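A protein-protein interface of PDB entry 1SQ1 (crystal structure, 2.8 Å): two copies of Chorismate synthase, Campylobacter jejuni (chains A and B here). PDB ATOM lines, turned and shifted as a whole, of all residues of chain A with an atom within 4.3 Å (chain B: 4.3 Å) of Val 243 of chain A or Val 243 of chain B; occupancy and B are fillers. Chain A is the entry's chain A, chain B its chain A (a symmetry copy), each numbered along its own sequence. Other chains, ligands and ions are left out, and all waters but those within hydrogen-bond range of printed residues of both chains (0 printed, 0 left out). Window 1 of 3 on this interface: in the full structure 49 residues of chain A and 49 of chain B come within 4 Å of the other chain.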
ATOM      1  N   LEU A 234      17.562  28.107 -10.822  1.00  0.00           N
ATOM      2  CA  LEU A 234      16.232  28.487 -10.362  1.00  0.00           C
ATOM      3  C   LEU A 234      15.355  27.271  -9.991  1.00  0.00           C
ATOM      4  O   LEU A 234      14.782  27.234  -8.893  1.00  0.00           O
ATOM      5  CB  LEU A 234      15.542  29.362 -11.420  1.00  0.00           C
ATOM      6  CG  LEU A 234      16.174  30.754 -11.621  1.00  0.00           C
ATOM      7  CD1 LEU A 234      15.490  31.552 -12.756  1.00  0.00           C
ATOM      8  CD2 LEU A 234      16.070  31.528 -10.312  1.00  0.00           C
ATOM      9  N   MET A 235      15.242  26.281 -10.885  1.00  0.00           N
ATOM     10  CA  MET A 235      14.453  25.063 -10.596  1.00  0.00           C
ATOM     11  C   MET A 235      15.018  24.417  -9.338  1.00  0.00           C
ATOM     12  O   MET A 235      14.286  23.813  -8.558  1.00  0.00           O
ATOM     13  CB  MET A 235      14.555  24.038 -11.738  1.00  0.00           C
ATOM     14  CG  MET A 235      13.538  24.153 -12.877  1.00  0.00           C
ATOM     15  SD  MET A 235      11.718  23.717 -12.391  1.00  0.00           S
ATOM     16  CE  MET A 235      12.125  22.577 -10.893  1.00  0.00           C
ATOM     17  N   VAL A 240      10.354  25.473  -6.106  1.00  0.00           N
ATOM     18  CA  VAL A 240      10.172  25.872  -7.495  1.00  0.00           C
ATOM     19  C   VAL A 240       9.700  24.733  -8.380  1.00  0.00           C
ATOM     20  O   VAL A 240      10.281  23.647  -8.376  1.00  0.00           O
ATOM     21  CB  VAL A 240      11.461  26.467  -8.083  1.00  0.00           C
ATOM     22  CG1 VAL A 240      11.275  26.722  -9.568  1.00  0.00           C
ATOM     23  CG2 VAL A 240      11.799  27.777  -7.374  1.00  0.00           C
ATOM     24  N   ALA A 242       8.369  25.637 -11.796  1.00  0.00           N
ATOM     25  CA  ALA A 242       8.345  26.121 -13.171  1.00  0.00           C
ATOM     26  C   ALA A 242       9.270  27.318 -13.362  1.00  0.00           C
ATOM     27  O   ALA A 242       9.491  28.109 -12.442  1.00  0.00           O
ATOM     28  CB  ALA A 242       6.927  26.484 -13.579  1.00  0.00           C
ATOM     29  N   VAL A 243       9.802  27.435 -14.573  1.00  0.00           N
ATOM     30  CA  VAL A 243      10.705  28.517 -14.921  1.00  0.00           C
ATOM     31  C   VAL A 243      10.434  29.036 -16.317  1.00  0.00           C
ATOM     32  O   VAL A 243      10.325  28.258 -17.277  1.00  0.00           O
ATOM     33  CB  VAL A 243      12.139  28.059 -14.889  1.00  0.00           C
ATOM     34  CG1 VAL A 243      13.041  29.201 -15.266  1.00  0.00           C
ATOM     35  CG2 VAL A 243      12.471  27.531 -13.520  1.00  0.00           C
ATOM     36  N   GLU A 244      10.331  30.357 -16.429  1.00  0.00           N
ATOM     37  CA  GLU A 244      10.070  30.978 -17.721  1.00  0.00           C
ATOM     38  C   GLU A 244      11.110  32.003 -18.127  1.00  0.00           C
ATOM     39  O   GLU A 244      11.645  32.741 -17.301  1.00  0.00           O
ATOM     40  CB  GLU A 244       8.712  31.676 -17.729  1.00  0.00           C
ATOM     41  CG  GLU A 244       7.522  30.754 -17.787  1.00  0.00           C
ATOM     42  CD  GLU A 244       6.242  31.521 -17.979  1.00  0.00           C
ATOM     43  OE1 GLU A 244       5.936  32.385 -17.132  1.00  0.00           O
ATOM     44  OE2 GLU A 244       5.546  31.262 -18.981  1.00  0.00           O
ATOM     45  N   LYS A 289      11.168  34.235 -14.984  1.00  0.00           N
ATOM     46  CA  LYS A 289      10.076  34.080 -14.045  1.00  0.00           C
ATOM     47  C   LYS A 289      10.165  32.732 -13.353  1.00  0.00           C
ATOM     48  O   LYS A 289      10.265  31.699 -14.016  1.00  0.00           O
ATOM     49  CB  LYS A 289       8.733  34.227 -14.756  1.00  0.00           C
ATOM     50  CG  LYS A 289       8.591  35.470 -15.612  1.00  0.00           C
ATOM     51  CD  LYS A 289       7.164  35.591 -16.072  1.00  0.00           C
ATOM     52  CE  LYS A 289       6.994  36.603 -17.192  1.00  0.00           C
ATOM     53  NZ  LYS A 289       7.630  36.124 -18.465  1.00  0.00           N
ATOM     54  N   LEU B 234      16.561  20.534 -20.815  1.00  0.00           N
ATOM     55  CA  LEU B 234      15.397  20.919 -21.604  1.00  0.00           C
ATOM     56  C   LEU B 234      15.456  22.387 -22.083  1.00  0.00           C
ATOM     57  O   LEU B 234      15.279  22.653 -23.281  1.00  0.00           O
ATOM     58  CB  LEU B 234      14.112  20.651 -20.808  1.00  0.00           C
ATOM     59  CG  LEU B 234      13.801  19.160 -20.564  1.00  0.00           C
ATOM     60  CD1 LEU B 234      12.544  18.957 -19.685  1.00  0.00           C
ATOM     61  CD2 LEU B 234      13.601  18.478 -21.913  1.00  0.00           C
ATOM     62  N   MET B 235      15.698  23.336 -21.173  1.00  0.00           N
ATOM     63  CA  MET B 235      15.809  24.762 -21.551  1.00  0.00           C
ATOM     64  C   MET B 235      16.916  24.896 -22.588  1.00  0.00           C
ATOM     65  O   MET B 235      16.849  25.745 -23.474  1.00  0.00           O
ATOM     66  CB  MET B 235      16.184  25.641 -20.346  1.00  0.00           C
ATOM     67  CG  MET B 235      15.037  26.190 -19.493  1.00  0.00           C
ATOM     68  SD  MET B 235      13.938  27.520 -20.364  1.00  0.00           S
ATOM     69  CE  MET B 235      15.249  28.135 -21.636  1.00  0.00           C
ATOM     70  N   VAL B 240      13.374  26.357 -26.905  1.00  0.00           N
ATOM     71  CA  VAL B 240      12.677  26.227 -25.632  1.00  0.00           C
ATOM     72  C   VAL B 240      12.718  27.498 -24.804  1.00  0.00           C
ATOM     73  O   VAL B 240      13.782  28.079 -24.590  1.00  0.00           O
ATOM     74  CB  VAL B 240      13.240  25.064 -24.799  1.00  0.00           C
ATOM     75  CG1 VAL B 240      12.598  25.063 -23.423  1.00  0.00           C
ATOM     76  CG2 VAL B 240      12.956  23.737 -25.501  1.00  0.00           C
ATOM     77  N   ALA B 242      10.343  27.730 -21.877  1.00  0.00           N
ATOM     78  CA  ALA B 242       9.730  27.441 -20.587  1.00  0.00           C
ATOM     79  C   ALA B 242       9.764  25.951 -20.269  1.00  0.00           C
ATOM     80  O   ALA B 242       9.723  25.104 -21.165  1.00  0.00           O
ATOM     81  CB  ALA B 242       8.299  27.952 -20.555  1.00  0.00           C
ATOM     82  N   VAL B 243       9.837  25.648 -18.978  1.00  0.00           N
ATOM     83  CA  VAL B 243       9.879  24.277 -18.505  1.00  0.00           C
ATOM     84  C   VAL B 243       9.044  24.096 -17.256  1.00  0.00           C
ATOM     85  O   VAL B 243       9.157  24.873 -16.295  1.00  0.00           O
ATOM     86  CB  VAL B 243      11.285  23.863 -18.162  1.00  0.00           C
ATOM     87  CG1 VAL B 243      11.286  22.445 -17.665  1.00  0.00           C
ATOM     88  CG2 VAL B 243      12.167  24.019 -19.370  1.00  0.00           C
ATOM     89  N   GLU B 244       8.206  23.064 -17.268  1.00  0.00           N
ATOM     90  CA  GLU B 244       7.347  22.786 -16.124  1.00  0.00           C
ATOM     91  C   GLU B 244       7.516  21.391 -15.558  1.00  0.00           C
ATOM     92  O   GLU B 244       7.733  20.422 -16.284  1.00  0.00           O
ATOM     93  CB  GLU B 244       5.875  22.956 -16.489  1.00  0.00           C
ATOM     94  CG  GLU B 244       5.418  24.383 -16.649  1.00  0.00           C
ATOM     95  CD  GLU B 244       3.927  24.466 -16.824  1.00  0.00           C
ATOM     96  OE1 GLU B 244       3.406  23.856 -17.780  1.00  0.00           O
ATOM     97  OE2 GLU B 244       3.274  25.138 -16.000  1.00  0.00           O
ATOM     98  N   LYS B 289       7.078  19.274 -18.751  1.00  0.00           N
ATOM     99  CA  LYS B 289       6.514  19.937 -19.909  1.00  0.00           C
ATOM    100  C   LYS B 289       7.494  20.958 -20.459  1.00  0.00           C
ATOM    101  O   LYS B 289       7.986  21.810 -19.718  1.00  0.00           O
ATOM    102  CB  LYS B 289       5.191  20.609 -19.550  1.00  0.00           C
ATOM    103  CG  LYS B 289       4.188  19.717 -18.846  1.00  0.00           C
ATOM    104  CD  LYS B 289       2.871  20.437 -18.748  1.00  0.00           C
ATOM    105  CE  LYS B 289       1.910  19.771 -17.778  1.00  0.00           C
ATOM    106  NZ  LYS B 289       2.380  19.912 -16.359  1.00  0.00           N
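O of Val 243 of chain A sits at hydrogen-bond distance from N of Val 243 of chain B (3.2 Å).
Val 243 of chain B touches Ala 242 of chain A.
CA of Ala 242 of chain B touches O of Val 243 of chain A (3.5 Å).
Of the printed residues of chain B, Ala 242 of chain A touches Val 243 (3.5 Å).
Of the printed residues of chain B, Val 243 of chain A touches Ala 242 (3.5 Å) and Val 243 (3.2 Å).
Of the printed residues of chain A, Ala 242 of chain B touches Val 243 (3.5 Å).
The nearest printed residue of chain B that does not touch Val 243 of chain A is Met 235 of chain B (4.8 Å).
The nearest printed residue of chain A that does not touch Ala 242 of chain B is Glu 244 of chain A (4.01 Å).
Printed residues of chain B that touch a printed residue of chain A: Ala 242 and Val 243.
Hydrophobic or aromatic side chains of chain A that line the printed part of chain B: Ala 242.
Among the printed residues, no Asp or Glu carboxylate lies within 4 Å of a Lys or Arg side-chain nitrogen of the other chain.
Ala 242 of chain A touches Val 243 of chain B, and with the chains exchanged Val 243 of chain A touches Ala 242 of chain B.
Val 243 of chain B touches its own counterpart, Val 243 of chain A.
7 positions are printed for both chains.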
